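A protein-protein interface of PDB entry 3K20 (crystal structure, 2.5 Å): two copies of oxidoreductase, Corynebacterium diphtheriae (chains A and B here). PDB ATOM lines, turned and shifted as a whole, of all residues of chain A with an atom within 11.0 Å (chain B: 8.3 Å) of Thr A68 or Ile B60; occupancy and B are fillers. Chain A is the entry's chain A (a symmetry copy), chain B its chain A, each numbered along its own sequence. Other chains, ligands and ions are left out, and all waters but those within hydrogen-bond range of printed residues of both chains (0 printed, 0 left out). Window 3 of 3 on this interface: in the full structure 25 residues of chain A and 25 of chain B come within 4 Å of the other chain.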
ATOM      1  N   LEU A  59       1.499 -16.748  36.482  1.00  0.00           N
ATOM      2  CA  LEU A  59       1.113 -17.585  35.348  1.00  0.00           C
ATOM      3  C   LEU A  59       2.036 -17.306  34.169  1.00  0.00           C
ATOM      4  O   LEU A  59       1.801 -17.770  33.054  1.00  0.00           O
ATOM      5  CB  LEU A  59      -0.324 -17.296  34.923  1.00  0.00           C
ATOM      6  CG  LEU A  59      -1.434 -17.908  35.764  1.00  0.00           C
ATOM      7  CD1 LEU A  59      -2.777 -17.541  35.143  1.00  0.00           C
ATOM      8  CD2 LEU A  59      -1.256 -19.425  35.821  1.00  0.00           C
ATOM      9  N   ILE A  60       3.087 -16.535  34.430  1.00  0.00           N
ATOM     10  CA  ILE A  60       4.032 -16.163  33.398  1.00  0.00           C
ATOM     11  C   ILE A  60       4.561 -17.346  32.594  1.00  0.00           C
ATOM     12  O   ILE A  60       4.404 -17.382  31.378  1.00  0.00           O
ATOM     13  CB  ILE A  60       5.176 -15.340  34.012  1.00  0.00           C
ATOM     14  CG1 ILE A  60       4.660 -13.920  34.269  1.00  0.00           C
ATOM     15  CG2 ILE A  60       6.393 -15.343  33.103  1.00  0.00           C
ATOM     16  CD1 ILE A  60       5.658 -12.996  34.896  1.00  0.00           C
ATOM     17  N   PRO A  61       5.183 -18.338  33.251  1.00  0.00           N
ATOM     18  CA  PRO A  61       5.668 -19.454  32.439  1.00  0.00           C
ATOM     19  C   PRO A  61       4.588 -20.100  31.575  1.00  0.00           C
ATOM     20  O   PRO A  61       4.856 -20.506  30.444  1.00  0.00           O
ATOM     21  CB  PRO A  61       6.254 -20.418  33.477  1.00  0.00           C
ATOM     22  CG  PRO A  61       5.507 -20.101  34.718  1.00  0.00           C
ATOM     23  CD  PRO A  61       5.436 -18.589  34.679  1.00  0.00           C
ATOM     24  N   ASP A  62       3.367 -20.181  32.089  1.00  0.00           N
ATOM     25  CA  ASP A  62       2.283 -20.798  31.332  1.00  0.00           C
ATOM     26  C   ASP A  62       1.885 -19.957  30.120  1.00  0.00           C
ATOM     27  O   ASP A  62       1.520 -20.498  29.069  1.00  0.00           O
ATOM     28  CB  ASP A  62       1.079 -21.020  32.241  1.00  0.00           C
ATOM     29  CG  ASP A  62       1.438 -21.796  33.482  1.00  0.00           C
ATOM     30  OD1 ASP A  62       2.137 -21.245  34.366  1.00  0.00           O
ATOM     31  OD2 ASP A  62       1.028 -22.971  33.572  1.00  0.00           O
ATOM     32  N   LEU A  63       1.950 -18.637  30.278  1.00  0.00           N
ATOM     33  CA  LEU A  63       1.609 -17.707  29.208  1.00  0.00           C
ATOM     34  C   LEU A  63       2.739 -17.674  28.186  1.00  0.00           C
ATOM     35  O   LEU A  63       2.498 -17.603  26.980  1.00  0.00           O
ATOM     36  CB  LEU A  63       1.378 -16.310  29.789  1.00  0.00           C
ATOM     37  CG  LEU A  63      -0.058 -15.856  30.089  1.00  0.00           C
ATOM     38  CD1 LEU A  63      -1.013 -17.034  30.158  1.00  0.00           C
ATOM     39  CD2 LEU A  63      -0.065 -15.079  31.393  1.00  0.00           C
ATOM     40  N   MET A  64       3.972 -17.720  28.683  1.00  0.00           N
ATOM     41  CA  MET A  64       5.159 -17.726  27.842  1.00  0.00           C
ATOM     42  C   MET A  64       5.098 -18.992  26.995  1.00  0.00           C
ATOM     43  O   MET A  64       5.467 -18.990  25.820  1.00  0.00           O
ATOM     44  CB  MET A  64       6.409 -17.712  28.735  1.00  0.00           C
ATOM     45  CG  MET A  64       7.726 -18.083  28.065  1.00  0.00           C
ATOM     46  SD  MET A  64       8.176 -19.815  28.323  1.00  0.00           S
ATOM     47  CE  MET A  64       8.068 -20.471  26.644  1.00  0.00           C
ATOM     48  N   THR A  65       4.608 -20.069  27.593  1.00  0.00           N
ATOM     49  CA  THR A  65       4.486 -21.339  26.896  1.00  0.00           C
ATOM     50  C   THR A  65       3.383 -21.277  25.841  1.00  0.00           C
ATOM     51  O   THR A  65       3.543 -21.787  24.733  1.00  0.00           O
ATOM     52  CB  THR A  65       4.177 -22.490  27.886  1.00  0.00           C
ATOM     53  OG1 THR A  65       5.319 -22.718  28.720  1.00  0.00           O
ATOM     54  CG2 THR A  65       3.822 -23.772  27.140  1.00  0.00           C
ATOM     55  N   ALA A  66       2.266 -20.647  26.187  1.00  0.00           N
ATOM     56  CA  ALA A  66       1.140 -20.536  25.266  1.00  0.00           C
ATOM     57  C   ALA A  66       1.482 -19.688  24.047  1.00  0.00           C
ATOM     58  O   ALA A  66       0.775 -19.728  23.040  1.00  0.00           O
ATOM     59  CB  ALA A  66      -0.069 -19.958  25.984  1.00  0.00           C
ATOM     60  N   MET A  67       2.560 -18.917  24.139  1.00  0.00           N
ATOM     61  CA  MET A  67       2.970 -18.078  23.022  1.00  0.00           C
ATOM     62  C   MET A  67       3.766 -18.886  22.002  1.00  0.00           C
ATOM     63  O   MET A  67       3.683 -18.636  20.801  1.00  0.00           O
ATOM     64  CB  MET A  67       3.808 -16.890  23.512  1.00  0.00           C
ATOM     65  CG  MET A  67       3.016 -15.843  24.298  1.00  0.00           C
ATOM     66  SD  MET A  67       1.433 -15.157  23.373  1.00  0.00           S
ATOM     67  CE  MET A  67       2.084 -13.416  22.845  1.00  0.00           C
ATOM     68  N   THR A  68       4.519 -19.867  22.489  1.00  0.00           N
ATOM     69  CA  THR A  68       5.338 -20.712  21.626  1.00  0.00           C
ATOM     70  C   THR A  68       4.802 -22.137  21.484  1.00  0.00           C
ATOM     71  O   THR A  68       5.525 -23.037  21.070  1.00  0.00           O
ATOM     72  CB  THR A  68       6.789 -20.771  22.152  1.00  0.00           C
ATOM     73  OG1 THR A  68       6.794 -21.190  23.523  1.00  0.00           O
ATOM     74  CG2 THR A  68       7.436 -19.398  22.053  1.00  0.00           C
ATOM     75  N   THR A  69       3.535 -22.336  21.823  1.00  0.00           N
ATOM     76  CA  THR A  69       2.902 -23.649  21.728  1.00  0.00           C
ATOM     77  C   THR A  69       1.400 -23.438  21.824  1.00  0.00           C
ATOM     78  O   THR A  69       0.897 -23.002  22.853  1.00  0.00           O
ATOM     79  CB  THR A  69       3.350 -24.578  22.872  1.00  0.00           C
ATOM     80  OG1 THR A  69       4.749 -24.852  22.745  1.00  0.00           O
ATOM     81  CG2 THR A  69       2.565 -25.884  22.839  1.00  0.00           C
ATOM     82  N   ARG A  70       0.683 -23.751  20.752  1.00  0.00           N
ATOM     83  CA  ARG A  70      -0.760 -23.556  20.736  1.00  0.00           C
ATOM     84  C   ARG A  70      -1.454 -24.267  21.893  1.00  0.00           C
ATOM     85  O   ARG A  70      -2.576 -23.910  22.263  1.00  0.00           O
ATOM     86  CB  ARG A  70      -1.356 -24.031  19.402  1.00  0.00           C
ATOM     87  CG  ARG A  70      -1.626 -25.534  19.311  1.00  0.00           C
ATOM     88  CD  ARG A  70      -2.285 -25.891  17.981  1.00  0.00           C
ATOM     89  NE  ARG A  70      -3.006 -27.162  18.034  1.00  0.00           N
ATOM     90  CZ  ARG A  70      -2.447 -28.348  18.270  1.00  0.00           C
ATOM     91  NH1 ARG A  70      -1.139 -28.441  18.478  1.00  0.00           N
ATOM     92  NH2 ARG A  70      -3.198 -29.443  18.298  1.00  0.00           N
ATOM     93  N   VAL A  71      -0.791 -25.270  22.462  1.00  0.00           N
ATOM     94  CA  VAL A  71      -1.369 -26.025  23.572  1.00  0.00           C
ATOM     95  C   VAL A  71      -1.089 -25.374  24.926  1.00  0.00           C
ATOM     96  O   VAL A  71       0.041 -24.980  25.230  1.00  0.00           O
ATOM     97  CB  VAL A  71      -0.854 -27.488  23.588  1.00  0.00           C
ATOM     98  CG1 VAL A  71      -1.430 -28.230  24.786  1.00  0.00           C
ATOM     99  CG2 VAL A  71      -1.252 -28.195  22.288  1.00  0.00           C
ATOM    100  N   HIS A  72      -2.138 -25.265  25.732  1.00  0.00           N
ATOM    101  CA  HIS A  72      -2.040 -24.654  27.049  1.00  0.00           C
ATOM    102  C   HIS A  72      -1.666 -25.686  28.109  1.00  0.00           C
ATOM    103  O   HIS A  72      -2.030 -26.861  28.007  1.00  0.00           O
ATOM    104  CB  HIS A  72      -3.380 -24.022  27.430  1.00  0.00           C
ATOM    105  CG  HIS A  72      -3.908 -23.049  26.419  1.00  0.00           C
ATOM    106  ND1 HIS A  72      -3.313 -21.830  26.176  1.00  0.00           N
ATOM    107  CD2 HIS A  72      -4.984 -23.113  25.600  1.00  0.00           C
ATOM    108  CE1 HIS A  72      -4.000 -21.182  25.250  1.00  0.00           C
ATOM    109  NE2 HIS A  72      -5.018 -21.941  24.886  1.00  0.00           N
ATOM    110  N   THR A  73      -0.941 -25.248  29.130  1.00  0.00           N
ATOM    111  CA  THR A  73      -0.572 -26.154  30.204  1.00  0.00           C
ATOM    112  C   THR A  73      -1.849 -26.579  30.925  1.00  0.00           C
ATOM    113  O   THR A  73      -2.927 -26.030  30.678  1.00  0.00           O
ATOM    114  CB  THR A  73       0.349 -25.473  31.212  1.00  0.00           C
ATOM    115  OG1 THR A  73      -0.358 -24.403  31.856  1.00  0.00           O
ATOM    116  CG2 THR A  73       1.580 -24.927  30.510  1.00  0.00           C
ATOM    117  N   LEU A  76      -3.084 -23.805  33.257  1.00  0.00           N
ATOM    118  CA  LEU A  76      -3.757 -22.738  32.523  1.00  0.00           C
ATOM    119  C   LEU A  76      -5.130 -23.168  32.031  1.00  0.00           C
ATOM    120  O   LEU A  76      -6.085 -22.398  32.080  1.00  0.00           O
ATOM    121  CB  LEU A  76      -2.883 -22.291  31.337  1.00  0.00           C
ATOM    122  CG  LEU A  76      -3.396 -21.165  30.439  1.00  0.00           C
ATOM    123  CD1 LEU A  76      -3.659 -19.919  31.266  1.00  0.00           C
ATOM    124  CD2 LEU A  76      -2.370 -20.877  29.363  1.00  0.00           C
ATOM    125  N   LEU A 103       1.216  -8.031  29.842  1.00  0.00           N
ATOM    126  CA  LEU A 103       0.909  -9.318  30.463  1.00  0.00           C
ATOM    127  C   LEU A 103      -0.600  -9.480  30.609  1.00  0.00           C
ATOM    128  O   LEU A 103      -1.148 -10.573  30.409  1.00  0.00           O
ATOM    129  CB  LEU A 103       1.569  -9.420  31.838  1.00  0.00           C
ATOM    130  CG  LEU A 103       1.258 -10.689  32.639  1.00  0.00           C
ATOM    131  CD1 LEU A 103       1.765 -11.938  31.920  1.00  0.00           C
ATOM    132  CD2 LEU A 103       1.907 -10.567  34.000  1.00  0.00           C
ATOM    133  N   MET A 106      -2.069 -10.159  27.164  1.00  0.00           N
ATOM    134  CA  MET A 106      -1.657 -11.506  26.783  1.00  0.00           C
ATOM    135  C   MET A 106      -2.575 -12.577  27.361  1.00  0.00           C
ATOM    136  O   MET A 106      -2.911 -13.555  26.687  1.00  0.00           O
ATOM    137  CB  MET A 106      -0.229 -11.768  27.248  1.00  0.00           C
ATOM    138  CG  MET A 106       0.343 -13.063  26.721  1.00  0.00           C
ATOM    139  SD  MET A 106       2.150 -13.358  27.351  1.00  0.00           S
ATOM    140  CE  MET A 106       3.066 -11.832  26.560  1.00  0.00           C
ATOM    141  N   ILE A 110      -4.896 -15.180  24.997  1.00  0.00           N
ATOM    142  CA  ILE A 110      -4.907 -16.623  25.169  1.00  0.00           C
ATOM    143  C   ILE A 110      -6.286 -17.272  25.328  1.00  0.00           C
ATOM    144  O   ILE A 110      -6.409 -18.490  25.213  1.00  0.00           O
ATOM    145  CB  ILE A 110      -4.021 -16.998  26.385  1.00  0.00           C
ATOM    146  CG1 ILE A 110      -2.779 -17.726  25.887  1.00  0.00           C
ATOM    147  CG2 ILE A 110      -4.819 -17.794  27.426  1.00  0.00           C
ATOM    148  CD1 ILE A 110      -1.922 -16.895  24.933  1.00  0.00           C
ATOM    149  N   GLY B  20       4.536 -10.945  15.096  1.00  0.00           N
ATOM    150  CA  GLY B  20       3.750 -12.078  14.643  1.00  0.00           C
ATOM    151  C   GLY B  20       4.188 -13.362  15.326  1.00  0.00           C
ATOM    152  O   GLY B  20       5.318 -13.468  15.803  1.00  0.00           O
ATOM    153  N   LEU B  21       3.296 -14.346  15.372  1.00  0.00           N
ATOM    154  CA  LEU B  21       3.612 -15.621  16.010  1.00  0.00           C
ATOM    155  C   LEU B  21       3.636 -16.802  15.039  1.00  0.00           C
ATOM    156  O   LEU B  21       4.343 -17.789  15.269  1.00  0.00           O
ATOM    157  CB  LEU B  21       2.610 -15.898  17.132  1.00  0.00           C
ATOM    158  CG  LEU B  21       3.066 -15.583  18.562  1.00  0.00           C
ATOM    159  CD1 LEU B  21       3.770 -14.233  18.626  1.00  0.00           C
ATOM    160  CD2 LEU B  21       1.848 -15.618  19.477  1.00  0.00           C
ATOM    161  N   GLU B  55      12.152 -10.020  15.714  1.00  0.00           N
ATOM    162  CA  GLU B  55      10.919 -10.787  15.838  1.00  0.00           C
ATOM    163  C   GLU B  55      10.733 -10.976  17.345  1.00  0.00           C
ATOM    164  O   GLU B  55      11.560 -11.612  18.003  1.00  0.00           O
ATOM    165  CB  GLU B  55      11.050 -12.144  15.141  1.00  0.00           C
ATOM    166  CG  GLU B  55      11.027 -12.069  13.622  1.00  0.00           C
ATOM    167  CD  GLU B  55       9.617 -12.082  13.030  1.00  0.00           C
ATOM    168  OE1 GLU B  55       8.668 -11.582  13.677  1.00  0.00           O
ATOM    169  OE2 GLU B  55       9.461 -12.580  11.891  1.00  0.00           O
ATOM    170  N   LEU B  56       9.664 -10.401  17.893  1.00  0.00           N
ATOM    171  CA  LEU B  56       9.392 -10.487  19.326  1.00  0.00           C
ATOM    172  C   LEU B  56       9.215 -11.906  19.857  1.00  0.00           C
ATOM    173  O   LEU B  56       9.542 -12.187  21.011  1.00  0.00           O
ATOM    174  CB  LEU B  56       8.158  -9.658  19.679  1.00  0.00           C
ATOM    175  CG  LEU B  56       8.303  -8.150  19.506  1.00  0.00           C
ATOM    176  CD1 LEU B  56       7.031  -7.478  19.991  1.00  0.00           C
ATOM    177  CD2 LEU B  56       9.513  -7.642  20.291  1.00  0.00           C
ATOM    178  N   SER B  57       8.698 -12.799  19.024  1.00  0.00           N
ATOM    179  CA  SER B  57       8.498 -14.180  19.441  1.00  0.00           C
ATOM    180  C   SER B  57       9.836 -14.844  19.771  1.00  0.00           C
ATOM    181  O   SER B  57       9.867 -15.914  20.369  1.00  0.00           O
ATOM    182  CB  SER B  57       7.791 -14.967  18.335  1.00  0.00           C
ATOM    183  OG  SER B  57       8.606 -15.046  17.172  1.00  0.00           O
ATOM    184  N   GLU B  58      10.942 -14.216  19.390  1.00  0.00           N
ATOM    185  CA  GLU B  58      12.258 -14.782  19.665  1.00  0.00           C
ATOM    186  C   GLU B  58      12.911 -14.096  20.858  1.00  0.00           C
ATOM    187  O   GLU B  58      14.075 -14.339  21.166  1.00  0.00           O
ATOM    188  CB  GLU B  58      13.151 -14.667  18.428  1.00  0.00           C
ATOM    189  CG  GLU B  58      12.466 -15.180  17.165  1.00  0.00           C
ATOM    190  CD  GLU B  58      13.358 -15.151  15.929  1.00  0.00           C
ATOM    191  OE1 GLU B  58      14.040 -14.126  15.695  1.00  0.00           O
ATOM    192  OE2 GLU B  58      13.364 -16.156  15.181  1.00  0.00           O
ATOM    193  N   LEU B  59      12.160 -13.220  21.516  1.00  0.00           N
ATOM    194  CA  LEU B  59      12.655 -12.516  22.697  1.00  0.00           C
ATOM    195  C   LEU B  59      11.794 -12.870  23.902  1.00  0.00           C
ATOM    196  O   LEU B  59      11.917 -12.270  24.970  1.00  0.00           O
ATOM    197  CB  LEU B  59      12.607 -11.005  22.489  1.00  0.00           C
ATOM    198  CG  LEU B  59      13.710 -10.384  21.645  1.00  0.00           C
ATOM    199  CD1 LEU B  59      13.505  -8.873  21.605  1.00  0.00           C
ATOM    200  CD2 LEU B  59      15.073 -10.733  22.244  1.00  0.00           C
ATOM    201  N   ILE B  60      10.916 -13.848  23.715  1.00  0.00           N
ATOM    202  CA  ILE B  60      10.011 -14.270  24.764  1.00  0.00           C
ATOM    203  C   ILE B  60      10.704 -14.568  26.089  1.00  0.00           C
ATOM    204  O   ILE B  60      10.383 -13.954  27.101  1.00  0.00           O
ATOM    205  CB  ILE B  60       9.175 -15.466  24.282  1.00  0.00           C
ATOM    206  CG1 ILE B  60       8.086 -14.940  23.340  1.00  0.00           C
ATOM    207  CG2 ILE B  60       8.586 -16.224  25.458  1.00  0.00           C
ATOM    208  CD1 ILE B  60       7.197 -15.997  22.759  1.00  0.00           C
ATOM    209  N   PRO B  61      11.670 -15.500  26.109  1.00  0.00           N
ATOM    210  CA  PRO B  61      12.309 -15.748  27.402  1.00  0.00           C
ATOM    211  C   PRO B  61      12.887 -14.494  28.051  1.00  0.00           C
ATOM    212  O   PRO B  61      12.829 -14.342  29.272  1.00  0.00           O
ATOM    213  CB  PRO B  61      13.381 -16.793  27.071  1.00  0.00           C
ATOM    214  CG  PRO B  61      13.673 -16.560  25.636  1.00  0.00           C
ATOM    215  CD  PRO B  61      12.297 -16.316  25.057  1.00  0.00           C
ATOM    216  N   ASP B  62      13.427 -13.587  27.246  1.00  0.00           N
ATOM    217  CA  ASP B  62      14.013 -12.367  27.792  1.00  0.00           C
ATOM    218  C   ASP B  62      12.953 -11.438  28.381  1.00  0.00           C
ATOM    219  O   ASP B  62      13.198 -10.754  29.381  1.00  0.00           O
ATOM    220  CB  ASP B  62      14.804 -11.645  26.707  1.00  0.00           C
ATOM    221  CG  ASP B  62      15.825 -12.541  26.054  1.00  0.00           C
ATOM    222  OD1 ASP B  62      15.434 -13.466  25.301  1.00  0.00           O
ATOM    223  OD2 ASP B  62      17.030 -12.329  26.303  1.00  0.00           O
ATOM    224  N   LEU B  63      11.781 -11.417  27.751  1.00  0.00           N
ATOM    225  CA  LEU B  63      10.670 -10.587  28.202  1.00  0.00           C
ATOM    226  C   LEU B  63      10.032 -11.218  29.434  1.00  0.00           C
ATOM    227  O   LEU B  63       9.639 -10.520  30.369  1.00  0.00           O
ATOM    228  CB  LEU B  63       9.636 -10.451  27.082  1.00  0.00           C
ATOM    229  CG  LEU B  63       9.670  -9.205  26.183  1.00  0.00           C
ATOM    230  CD1 LEU B  63      11.004  -8.487  26.276  1.00  0.00           C
ATOM    231  CD2 LEU B  63       9.381  -9.624  24.754  1.00  0.00           C
ATOM    232  N   MET B  64       9.932 -12.544  29.420  1.00  0.00           N
ATOM    233  CA  MET B  64       9.374 -13.303  30.529  1.00  0.00           C
ATOM    234  C   MET B  64      10.275 -13.054  31.735  1.00  0.00           C
ATOM    235  O   MET B  64       9.805 -12.932  32.867  1.00  0.00           O
ATOM    236  CB  MET B  64       9.343 -14.792  30.156  1.00  0.00           C
ATOM    237  CG  MET B  64       9.143 -15.775  31.302  1.00  0.00           C
ATOM    238  SD  MET B  64      10.699 -16.475  31.900  1.00  0.00           S
ATOM    239  CE  MET B  64      10.784 -15.793  33.570  1.00  0.00           C
ATOM    240  N   THR B  65      11.573 -12.956  31.481  1.00  0.00           N
ATOM    241  CA  THR B  65      12.540 -12.710  32.539  1.00  0.00           C
ATOM    242  C   THR B  65      12.414 -11.284  33.070  1.00  0.00           C
ATOM    243  O   THR B  65      12.484 -11.053  34.276  1.00  0.00           O
ATOM    244  CB  THR B  65      13.986 -12.938  32.034  1.00  0.00           C
ATOM    245  OG1 THR B  65      14.183 -14.333  31.771  1.00  0.00           O
ATOM    246  CG2 THR B  65      15.005 -12.462  33.064  1.00  0.00           C
ATOM    247  N   ALA B  66      12.223 -10.328  32.166  1.00  0.00           N
ATOM    248  CA  ALA B  66      12.103  -8.927  32.556  1.00  0.00           C
ATOM    249  C   ALA B  66      10.852  -8.672  33.386  1.00  0.00           C
ATOM    250  O   ALA B  66      10.738  -7.638  34.043  1.00  0.00           O
ATOM    251  CB  ALA B  66      12.102  -8.040  31.321  1.00  0.00           C
ATOM    252  N   MET B  67       9.911  -9.610  33.353  1.00  0.00           N
ATOM    253  CA  MET B  67       8.684  -9.459  34.121  1.00  0.00           C
ATOM    254  C   MET B  67       8.899  -9.876  35.572  1.00  0.00           C
ATOM    255  O   MET B  67       8.304  -9.306  36.485  1.00  0.00           O
ATOM    256  CB  MET B  67       7.550 -10.287  33.505  1.00  0.00           C
ATOM    257  CG  MET B  67       7.039  -9.757  32.163  1.00  0.00           C
ATOM    258  SD  MET B  67       6.503  -7.873  32.184  1.00  0.00           S
ATOM    259  CE  MET B  67       4.582  -8.074  32.171  1.00  0.00           C
ATOM    260  N   THR B  73      18.167  -9.042  30.389  1.00  0.00           N
ATOM    261  CA  THR B  73      19.249  -9.898  29.935  1.00  0.00           C
ATOM    262  C   THR B  73      20.185  -9.057  29.068  1.00  0.00           C
ATOM    263  O   THR B  73      19.867  -7.916  28.720  1.00  0.00           O
ATOM    264  CB  THR B  73      18.724 -11.059  29.096  1.00  0.00           C
ATOM    265  OG1 THR B  73      18.128 -10.547  27.895  1.00  0.00           O
ATOM    266  CG2 THR B  73      17.698 -11.851  29.885  1.00  0.00           C
ATOM    267  N   LYS B  75      21.117  -9.809  26.001  1.00  0.00           N
ATOM    268  CA  LYS B  75      20.546  -9.820  24.667  1.00  0.00           C
ATOM    269  C   LYS B  75      19.505  -8.710  24.535  1.00  0.00           C
ATOM    270  O   LYS B  75      19.445  -8.010  23.520  1.00  0.00           O
ATOM    271  CB  LYS B  75      19.917 -11.187  24.400  1.00  0.00           C
ATOM    272  CG  LYS B  75      19.402 -11.405  22.998  1.00  0.00           C
ATOM    273  CD  LYS B  75      18.896 -12.835  22.857  1.00  0.00           C
ATOM    274  CE  LYS B  75      18.263 -13.079  21.496  1.00  0.00           C
ATOM    275  NZ  LYS B  75      17.555 -14.390  21.450  1.00  0.00           N
ATOM    276  N   LEU B  76      18.702  -8.536  25.577  1.00  0.00           N
ATOM    277  CA  LEU B  76      17.654  -7.519  25.578  1.00  0.00           C
ATOM    278  C   LEU B  76      18.226  -6.119  25.728  1.00  0.00           C
ATOM    279  O   LEU B  76      17.773  -5.181  25.078  1.00  0.00           O
ATOM    280  CB  LEU B  76      16.650  -7.807  26.708  1.00  0.00           C
ATOM    281  CG  LEU B  76      15.457  -6.866  26.878  1.00  0.00           C
ATOM    282  CD1 LEU B  76      14.648  -6.813  25.594  1.00  0.00           C
ATOM    283  CD2 LEU B  76      14.596  -7.353  28.024  1.00  0.00           C
ATOM    284  N   LEU B 103       2.123  -9.426  23.754  1.00  0.00           N
ATOM    285  CA  LEU B 103       3.574  -9.527  23.621  1.00  0.00           C
ATOM    286  C   LEU B 103       4.141  -8.221  23.073  1.00  0.00           C
ATOM    287  O   LEU B 103       5.210  -7.761  23.496  1.00  0.00           O
ATOM    288  CB  LEU B 103       3.948 -10.677  22.687  1.00  0.00           C
ATOM    289  CG  LEU B 103       5.442 -10.843  22.391  1.00  0.00           C
ATOM    290  CD1 LEU B 103       6.229 -11.162  23.662  1.00  0.00           C
ATOM    291  CD2 LEU B 103       5.609 -11.954  21.378  1.00  0.00           C
ATOM    292  N   MET B 106       4.014  -5.607  25.838  1.00  0.00           N
ATOM    293  CA  MET B 106       5.021  -5.982  26.824  1.00  0.00           C
ATOM    294  C   MET B 106       6.413  -5.484  26.447  1.00  0.00           C
ATOM    295  O   MET B 106       7.172  -5.020  27.303  1.00  0.00           O
ATOM    296  CB  MET B 106       5.060  -7.498  26.984  1.00  0.00           C
ATOM    297  CG  MET B 106       5.933  -7.956  28.129  1.00  0.00           C
ATOM    298  SD  MET B 106       5.963  -9.886  28.282  1.00  0.00           S
ATOM    299  CE  MET B 106       4.088 -10.249  28.664  1.00  0.00           C
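Of chain B, only Ile B60 comes within 4 Å of Thr A68.
Ile B60 touches three residues of chain A.
No residue of chain A comes within 4 Å of Ser B57.
No residue of chain A comes within 4 Å of Leu B59.
No residue of chain A comes within 4 Å of Asp B62.
No residue of chain A comes within 4 Å of Leu B63.
Printed residues of chain A within 4 Å of Met B106: Leu A103 (3.8 Å) and Met A106 (2.8 Å).
Of the printed residues of chain B, Ile A60 touches Met B64 (3.3 Å) and Met B67 (3.6 Å).
Of the printed residues of chain B, Met A67 touches Leu B21 (3.8 Å), Ile B60 (3.6 Å) and Leu B103 (3.3 Å).
Of the printed residues of chain B, Leu A103 touches Met B67 (3.3 Å) and Met B106 (3.8 Å).
Of the printed residues of chain A, Leu B21 touches Met A67.
His A72 touches none of the printed residues of chain B.
The nearest residue of chain B that does not touch Thr A68 is Ser B57 (4.6 Å).
The nearest printed residue of chain A that does not touch Leu B103 is Leu A103 (6.3 Å).
Ile A60 touches Met B64, and with the chains exchanged Met A64 touches Ile B60.
Ile A60 touches Met B67, and with the chains exchanged Met A67 touches Ile B60.
Met A67 touches Leu B103, and with the chains exchanged Leu A103 touches Met B67.
Met A106 touches its own counterpart, Met B106.
Positions printed for both chains: 59, 60, 61, 62, 63, 64, 65, 66, 67, 73, 76, 103 and 106.
Of the 11 pairs that touch across the chains among the printed residues, 9 have their exchanged pair printed and touching as well.
Of the 20 printed residues of chain B, 6 touch a printed residue of chain A.
Hydrophobic or aromatic side chains of chain B within 4 Å of the printed part of chain A: Leu B21, Ile B60, Met B64, Met B67, Leu B103 and Met B106.
Of the 19 printed residues of chain A, 6 touch a printed residue of chain B.
Hydrophobic or aromatic side chains of chain A within 4 Å of the printed part of chain B: Ile A60, Met A64, Met A67, Leu A103 and Met A106.
The backbone carbonyl oxygen (O) of Met A64 is in hydrogen-bond range of the side-chain hydroxyl (OG1) of Thr A68 (3.4 Å).
Among the printed residues, merely in contact across the chains: Met A106 with Met B106, Met A64 with Ile B60, Ile A60 with Met B64, Leu A103 with Met B67, Met A67 with Leu B103, Thr A68 with Ile B60, Met A67 with Ile B60, Ile A60 with Met B67, Met A106 with Leu B103, Leu A103 with Met B106 and Met A67 with Leu B21.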
